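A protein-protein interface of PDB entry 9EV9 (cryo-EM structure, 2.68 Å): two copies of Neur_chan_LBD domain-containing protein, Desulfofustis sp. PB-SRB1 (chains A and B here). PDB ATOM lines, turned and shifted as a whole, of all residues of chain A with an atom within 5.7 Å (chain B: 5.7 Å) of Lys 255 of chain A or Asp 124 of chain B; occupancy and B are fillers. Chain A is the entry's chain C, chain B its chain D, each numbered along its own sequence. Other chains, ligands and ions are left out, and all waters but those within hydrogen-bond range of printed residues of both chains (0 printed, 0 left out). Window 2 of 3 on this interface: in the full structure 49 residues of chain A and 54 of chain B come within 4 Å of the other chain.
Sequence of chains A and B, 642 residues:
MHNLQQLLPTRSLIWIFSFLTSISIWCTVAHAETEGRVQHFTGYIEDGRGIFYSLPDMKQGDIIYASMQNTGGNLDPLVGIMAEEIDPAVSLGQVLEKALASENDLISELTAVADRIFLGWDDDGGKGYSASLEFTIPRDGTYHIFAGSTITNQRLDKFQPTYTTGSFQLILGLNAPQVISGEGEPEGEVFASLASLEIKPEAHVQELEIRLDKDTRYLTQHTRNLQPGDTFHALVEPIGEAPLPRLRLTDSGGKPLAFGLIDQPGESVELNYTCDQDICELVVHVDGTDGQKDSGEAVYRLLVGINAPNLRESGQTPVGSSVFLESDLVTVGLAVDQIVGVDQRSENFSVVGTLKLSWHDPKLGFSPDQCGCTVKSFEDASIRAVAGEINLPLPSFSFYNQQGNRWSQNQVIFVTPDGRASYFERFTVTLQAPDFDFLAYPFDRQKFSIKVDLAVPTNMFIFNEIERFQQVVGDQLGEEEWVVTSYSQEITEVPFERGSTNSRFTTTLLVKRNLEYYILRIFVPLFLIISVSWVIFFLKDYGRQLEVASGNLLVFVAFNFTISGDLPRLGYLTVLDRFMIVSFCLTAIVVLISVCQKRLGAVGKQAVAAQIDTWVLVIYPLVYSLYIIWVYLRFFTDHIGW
No position is printed for both chains. Of the 7 pairs that touch across the chains among the printed residues, none has its exchanged pair printed and touching as well.
The backbone NH (N) of Lys 255 of chain A is in hydrogen-bond range of the side-chain carboxylate (OD1) of Asp 251 of chain A (2.5 Å). N of Thr 150 of chain B lies within hydrogen-bond range of O of Asp 76 of chain B, at 3.4 Å. OD1 of Asp 251 of chain A lies within hydrogen-bond range of N of Gly 254 of chain A (2.9 Å). OD1 of Asp 251 of chain A lies close to N of Gly 253 of chain A, 3.3 Å away.
Of the printed residues of chain B, Lys 255 of chain A touches Asp 76 (3.4 Å), Asp 124 (2.4 Å), Tyr 129 (3.3 Å), Thr 152 (3.5 Å) and Asn 153 (3.8 Å). Of chain A, only Lys 255 (2.4 Å) comes within 4 Å of Asp 124 of chain B. Printed residues of chain B within 4 Å of Asp 251 of chain A: Tyr 129. Printed residues of chain A within 4 Å of Asn 153 of chain B: Gly 254 (2.6 Å) and Lys 255 (3.8 Å). Of the printed residues of chain A, Asp 76 of chain B touches Lys 255. Of the printed residues of chain A, Thr 152 of chain B touches Lys 255 (3.5 Å). Thr 250 of chain A touches none of the printed residues of chain B. Ser 130 of chain B touches none of the printed residues of chain A. The nearest printed residue of chain B that does not touch Lys 255 of chain A is Asp 123 of chain B (4.01 Å). The nearest printed residue of chain A that does not touch Asp 124 of chain B is Gln 277 of chain A (5.7 Å). The nearest printed residue of chain B that does not touch Asp 251 of chain A is Asn 153 of chain B (6.1 Å).
Among the printed residues, merely in contact across the chains: Lys 255 of chain A with Tyr 129 of chain B (3.3 Å), Lys 255 of chain A with Thr 152 of chain B (3.5 Å) and Lys 255 of chain A with Asn 153 of chain B (3.8 Å).
The side-chain amino group of Lys 255 of chain A is in salt-bridge range of the side-chain carboxylate of Asp 124 of chain B (2.4 Å). O of Gly 254 of chain A lies close to O of Asn 153 of chain B. OD2 of Asp 251 of chain A sits at hydrogen-bond distance from OH of Tyr 129 of chain B (2.9 Å). NZ of Lys 255 of chain A lies within salt-bridge range of OD2 of Asp 76 of chain B.
Printed residues of chain B that touch a printed residue of chain A: Asp 76, Asp 124, Tyr 129, Thr 152 and Asn 153. Along chain B the printed residues that touch a printed residue of chain A span positions 76 to 153.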
ATOM      1  N   LEU A 249      30.533  23.149  -8.514  1.00  0.00           N
ATOM      2  CA  LEU A 249      30.495  24.012  -7.342  1.00  0.00           C
ATOM      3  C   LEU A 249      30.137  23.186  -6.117  1.00  0.00           C
ATOM      4  O   LEU A 249      29.153  22.440  -6.134  1.00  0.00           O
ATOM      5  CB  LEU A 249      29.486  25.152  -7.527  1.00  0.00           C
ATOM      6  CG  LEU A 249      29.362  26.153  -6.379  1.00  0.00           C
ATOM      7  CD1 LEU A 249      30.670  26.898  -6.174  1.00  0.00           C
ATOM      8  CD2 LEU A 249      28.225  27.127  -6.632  1.00  0.00           C
ATOM      9  N   THR A 250      30.937  23.320  -5.061  1.00  0.00           N
ATOM     10  CA  THR A 250      30.722  22.617  -3.805  1.00  0.00           C
ATOM     11  C   THR A 250      30.944  23.579  -2.649  1.00  0.00           C
ATOM     12  O   THR A 250      31.594  24.617  -2.794  1.00  0.00           O
ATOM     13  CB  THR A 250      31.656  21.405  -3.655  1.00  0.00           C
ATOM     14  OG1 THR A 250      33.021  21.831  -3.758  1.00  0.00           O
ATOM     15  CG2 THR A 250      31.373  20.363  -4.725  1.00  0.00           C
ATOM     16  N   ASP A 251      30.397  23.224  -1.490  1.00  0.00           N
ATOM     17  CA  ASP A 251      30.566  24.031  -0.289  1.00  0.00           C
ATOM     18  C   ASP A 251      31.921  23.718   0.346  1.00  0.00           C
ATOM     19  O   ASP A 251      32.747  22.994  -0.214  1.00  0.00           O
ATOM     20  CB  ASP A 251      29.410  23.793   0.678  1.00  0.00           C
ATOM     21  CG  ASP A 251      29.466  22.429   1.330  1.00  0.00           C
ATOM     22  OD1 ASP A 251      29.936  21.475   0.675  1.00  0.00           O
ATOM     23  OD2 ASP A 251      29.042  22.312   2.499  1.00  0.00           O
ATOM     24  N   GLY A 253      32.454  21.864   2.842  1.00  0.00           N
ATOM     25  CA  GLY A 253      32.512  20.492   3.299  1.00  0.00           C
ATOM     26  C   GLY A 253      32.580  19.491   2.165  1.00  0.00           C
ATOM     27  O   GLY A 253      32.834  18.304   2.388  1.00  0.00           O
ATOM     28  N   GLY A 254      32.351  19.960   0.941  1.00  0.00           N
ATOM     29  CA  GLY A 254      32.370  19.110  -0.229  1.00  0.00           C
ATOM     30  C   GLY A 254      31.012  18.708  -0.761  1.00  0.00           C
ATOM     31  O   GLY A 254      30.950  17.973  -1.755  1.00  0.00           O
ATOM     32  N   LYS A 255      29.931  19.155  -0.139  1.00  0.00           N
ATOM     33  CA  LYS A 255      28.596  18.820  -0.619  1.00  0.00           C
ATOM     34  C   LYS A 255      28.348  19.490  -1.965  1.00  0.00           C
ATOM     35  O   LYS A 255      28.447  20.719  -2.067  1.00  0.00           O
ATOM     36  CB  LYS A 255      27.549  19.263   0.399  1.00  0.00           C
ATOM     37  CG  LYS A 255      26.577  18.177   0.818  1.00  0.00           C
ATOM     38  CD  LYS A 255      25.619  17.825  -0.305  1.00  0.00           C
ATOM     39  CE  LYS A 255      24.691  16.696   0.104  1.00  0.00           C
ATOM     40  NZ  LYS A 255      23.984  17.002   1.378  1.00  0.00           N
ATOM     41  N   PRO A 256      28.034  18.733  -3.013  1.00  0.00           N
ATOM     42  CA  PRO A 256      27.843  19.345  -4.332  1.00  0.00           C
ATOM     43  C   PRO A 256      26.619  20.246  -4.365  1.00  0.00           C
ATOM     44  O   PRO A 256      25.612  19.995  -3.700  1.00  0.00           O
ATOM     45  CB  PRO A 256      27.672  18.139  -5.261  1.00  0.00           C
ATOM     46  CG  PRO A 256      27.195  17.045  -4.369  1.00  0.00           C
ATOM     47  CD  PRO A 256      27.867  17.271  -3.052  1.00  0.00           C
ATOM     48  N   LEU A 257      26.721  21.309  -5.151  1.00  0.00           N
ATOM     49  CA  LEU A 257      25.639  22.278  -5.296  1.00  0.00           C
ATOM     50  C   LEU A 257      25.219  22.492  -6.742  1.00  0.00           C
ATOM     51  O   LEU A 257      24.025  22.655  -7.011  1.00  0.00           O
ATOM     52  CB  LEU A 257      26.050  23.621  -4.669  1.00  0.00           C
ATOM     53  CG  LEU A 257      26.328  23.594  -3.166  1.00  0.00           C
ATOM     54  CD1 LEU A 257      26.741  24.967  -2.666  1.00  0.00           C
ATOM     55  CD2 LEU A 257      25.113  23.091  -2.405  1.00  0.00           C
ATOM     56  N   GLN A 277      20.807  29.504   2.360  1.00  0.00           N
ATOM     57  CA  GLN A 277      21.135  29.498   3.775  1.00  0.00           C
ATOM     58  C   GLN A 277      21.570  30.890   4.234  1.00  0.00           C
ATOM     59  O   GLN A 277      21.773  31.807   3.434  1.00  0.00           O
ATOM     60  CB  GLN A 277      22.229  28.473   4.070  1.00  0.00           C
ATOM     61  CG  GLN A 277      21.793  27.021   3.916  1.00  0.00           C
ATOM     62  CD  GLN A 277      21.714  26.575   2.468  1.00  0.00           C
ATOM     63  OE1 GLN A 277      22.477  27.042   1.621  1.00  0.00           O
ATOM     64  NE2 GLN A 277      20.786  25.672   2.176  1.00  0.00           N
ATOM     65  N   ASP B  76      25.312  10.780   5.839  1.00  0.00           N
ATOM     66  CA  ASP B  76      24.524  11.857   5.251  1.00  0.00           C
ATOM     67  C   ASP B  76      23.094  11.372   5.046  1.00  0.00           C
ATOM     68  O   ASP B  76      22.836  10.606   4.104  1.00  0.00           O
ATOM     69  CB  ASP B  76      25.138  12.303   3.924  1.00  0.00           C
ATOM     70  CG  ASP B  76      24.794  13.734   3.572  1.00  0.00           C
ATOM     71  OD1 ASP B  76      23.723  14.211   3.996  1.00  0.00           O
ATOM     72  OD2 ASP B  76      25.601  14.384   2.878  1.00  0.00           O
ATOM     73  N   PRO B  77      22.143  11.783   5.883  1.00  0.00           N
ATOM     74  CA  PRO B  77      20.806  11.175   5.854  1.00  0.00           C
ATOM     75  C   PRO B  77      20.051  11.418   4.554  1.00  0.00           C
ATOM     76  O   PRO B  77      20.223  12.437   3.881  1.00  0.00           O
ATOM     77  CB  PRO B  77      20.094  11.844   7.033  1.00  0.00           C
ATOM     78  CG  PRO B  77      21.192  12.300   7.928  1.00  0.00           C
ATOM     79  CD  PRO B  77      22.308  12.697   7.020  1.00  0.00           C
ATOM     80  N   ASP B 122      13.523  13.885   0.641  1.00  0.00           N
ATOM     81  CA  ASP B 122      14.234  15.098   1.022  1.00  0.00           C
ATOM     82  C   ASP B 122      15.665  14.735   1.384  1.00  0.00           C
ATOM     83  O   ASP B 122      15.905  13.705   2.017  1.00  0.00           O
ATOM     84  CB  ASP B 122      13.560  15.807   2.200  1.00  0.00           C
ATOM     85  CG  ASP B 122      14.274  17.083   2.594  1.00  0.00           C
ATOM     86  OD1 ASP B 122      14.249  18.048   1.801  1.00  0.00           O
ATOM     87  OD2 ASP B 122      14.864  17.125   3.693  1.00  0.00           O
ATOM     88  N   ASP B 123      16.608  15.586   0.979  1.00  0.00           N
ATOM     89  CA  ASP B 123      18.028  15.348   1.229  1.00  0.00           C
ATOM     90  C   ASP B 123      18.553  16.215   2.367  1.00  0.00           C
ATOM     91  O   ASP B 123      19.042  15.682   3.365  1.00  0.00           O
ATOM     92  CB  ASP B 123      18.827  15.585  -0.054  1.00  0.00           C
ATOM     93  CG  ASP B 123      20.185  14.916  -0.029  1.00  0.00           C
ATOM     94  OD1 ASP B 123      20.724  14.684   1.073  1.00  0.00           O
ATOM     95  OD2 ASP B 123      20.716  14.616  -1.116  1.00  0.00           O
ATOM     96  N   ASP B 124      18.463  17.538   2.253  1.00  0.00           N
ATOM     97  CA  ASP B 124      19.148  18.460   3.155  1.00  0.00           C
ATOM     98  C   ASP B 124      18.216  19.550   3.668  1.00  0.00           C
ATOM     99  O   ASP B 124      18.620  20.700   3.851  1.00  0.00           O
ATOM    100  CB  ASP B 124      20.356  19.087   2.465  1.00  0.00           C
ATOM    101  CG  ASP B 124      21.380  18.059   2.037  1.00  0.00           C
ATOM    102  OD1 ASP B 124      21.612  17.100   2.802  1.00  0.00           O
ATOM    103  OD2 ASP B 124      21.951  18.206   0.938  1.00  0.00           O
ATOM    104  N   GLY B 125      16.957  19.204   3.925  1.00  0.00           N
ATOM    105  CA  GLY B 125      15.989  20.204   4.328  1.00  0.00           C
ATOM    106  C   GLY B 125      16.105  20.691   5.756  1.00  0.00           C
ATOM    107  O   GLY B 125      15.438  21.665   6.115  1.00  0.00           O
ATOM    108  N   GLY B 126      16.935  20.047   6.578  1.00  0.00           N
ATOM    109  CA  GLY B 126      17.061  20.381   7.971  1.00  0.00           C
ATOM    110  C   GLY B 126      18.341  21.123   8.289  1.00  0.00           C
ATOM    111  O   GLY B 126      19.003  21.689   7.409  1.00  0.00           O
ATOM    112  N   GLY B 128      21.907  21.604   8.695  1.00  0.00           N
ATOM    113  CA  GLY B 128      23.047  20.913   8.133  1.00  0.00           C
ATOM    114  C   GLY B 128      22.632  19.990   7.010  1.00  0.00           C
ATOM    115  O   GLY B 128      21.898  20.396   6.106  1.00  0.00           O
ATOM    116  N   TYR B 129      23.090  18.740   7.061  1.00  0.00           N
ATOM    117  CA  TYR B 129      22.775  17.744   6.047  1.00  0.00           C
ATOM    118  C   TYR B 129      21.593  16.865   6.440  1.00  0.00           C
ATOM    119  O   TYR B 129      21.311  15.874   5.760  1.00  0.00           O
ATOM    120  CB  TYR B 129      24.006  16.882   5.760  1.00  0.00           C
ATOM    121  CG  TYR B 129      25.171  17.645   5.174  1.00  0.00           C
ATOM    122  CD1 TYR B 129      24.973  18.816   4.460  1.00  0.00           C
ATOM    123  CD2 TYR B 129      26.472  17.192   5.332  1.00  0.00           C
ATOM    124  CE1 TYR B 129      26.035  19.513   3.923  1.00  0.00           C
ATOM    125  CE2 TYR B 129      27.539  17.882   4.800  1.00  0.00           C
ATOM    126  CZ  TYR B 129      27.317  19.042   4.098  1.00  0.00           C
ATOM    127  OH  TYR B 129      28.379  19.730   3.566  1.00  0.00           O
ATOM    128  N   SER B 130      20.894  17.215   7.518  1.00  0.00           N
ATOM    129  CA  SER B 130      19.762  16.428   7.985  1.00  0.00           C
ATOM    130  C   SER B 130      18.544  16.651   7.095  1.00  0.00           C
ATOM    131  O   SER B 130      18.370  17.725   6.511  1.00  0.00           O
ATOM    132  CB  SER B 130      19.427  16.790   9.429  1.00  0.00           C
ATOM    133  OG  SER B 130      19.088  18.161   9.545  1.00  0.00           O
ATOM    134  N   ALA B 131      17.705  15.628   6.995  1.00  0.00           N
ATOM    135  CA  ALA B 131      16.530  15.653   6.137  1.00  0.00           C
ATOM    136  C   ALA B 131      15.260  15.907   6.943  1.00  0.00           C
ATOM    137  O   ALA B 131      15.175  15.572   8.126  1.00  0.00           O
ATOM    138  CB  ALA B 131      16.393  14.338   5.368  1.00  0.00           C
ATOM    139  N   SER B 132      14.273  16.510   6.282  1.00  0.00           N
ATOM    140  CA  SER B 132      12.959  16.736   6.865  1.00  0.00           C
ATOM    141  C   SER B 132      11.924  16.682   5.752  1.00  0.00           C
ATOM    142  O   SER B 132      12.124  17.271   4.689  1.00  0.00           O
ATOM    143  CB  SER B 132      12.896  18.076   7.601  1.00  0.00           C
ATOM    144  OG  SER B 132      13.254  19.142   6.741  1.00  0.00           O
ATOM    145  N   THR B 150      22.634   9.048   1.124  1.00  0.00           N
ATOM    146  CA  THR B 150      22.702   9.614  -0.213  1.00  0.00           C
ATOM    147  C   THR B 150      24.109   9.460  -0.790  1.00  0.00           C
ATOM    148  O   THR B 150      25.024   8.940  -0.147  1.00  0.00           O
ATOM    149  CB  THR B 150      22.302  11.088  -0.192  1.00  0.00           C
ATOM    150  OG1 THR B 150      22.499  11.658  -1.491  1.00  0.00           O
ATOM    151  CG2 THR B 150      23.132  11.847   0.821  1.00  0.00           C
ATOM    152  N   ILE B 151      24.274   9.917  -2.027  1.00  0.00           N
ATOM    153  CA  ILE B 151      25.560   9.891  -2.716  1.00  0.00           C
ATOM    154  C   ILE B 151      26.151  11.292  -2.670  1.00  0.00           C
ATOM    155  O   ILE B 151      25.553  12.243  -3.188  1.00  0.00           O
ATOM    156  CB  ILE B 151      25.408   9.401  -4.164  1.00  0.00           C
ATOM    157  CG1 ILE B 151      24.820   7.992  -4.190  1.00  0.00           C
ATOM    158  CG2 ILE B 151      26.745   9.437  -4.879  1.00  0.00           C
ATOM    159  CD1 ILE B 151      24.591   7.457  -5.584  1.00  0.00           C
ATOM    160  N   THR B 152      27.331  11.422  -2.066  1.00  0.00           N
ATOM    161  CA  THR B 152      27.939  12.726  -1.839  1.00  0.00           C
ATOM    162  C   THR B 152      29.443  12.646  -2.058  1.00  0.00           C
ATOM    163  O   THR B 152      30.026  11.563  -2.131  1.00  0.00           O
ATOM    164  CB  THR B 152      27.662  13.251  -0.424  1.00  0.00           C
ATOM    165  OG1 THR B 152      28.092  12.285   0.541  1.00  0.00           O
ATOM    166  CG2 THR B 152      26.186  13.534  -0.227  1.00  0.00           C
ATOM    167  N   ASN B 153      30.058  13.820  -2.172  1.00  0.00           N
ATOM    168  CA  ASN B 153      31.507  13.972  -2.213  1.00  0.00           C
ATOM    169  C   ASN B 153      31.956  14.714  -0.961  1.00  0.00           C
ATOM    170  O   ASN B 153      31.301  15.670  -0.536  1.00  0.00           O
ATOM    171  CB  ASN B 153      31.943  14.730  -3.468  1.00  0.00           C
ATOM    172  CG  ASN B 153      33.440  14.929  -3.537  1.00  0.00           C
ATOM    173  OD1 ASN B 153      34.183  14.004  -3.864  1.00  0.00           O
ATOM    174  ND2 ASN B 153      33.893  16.138  -3.242  1.00  0.00           N
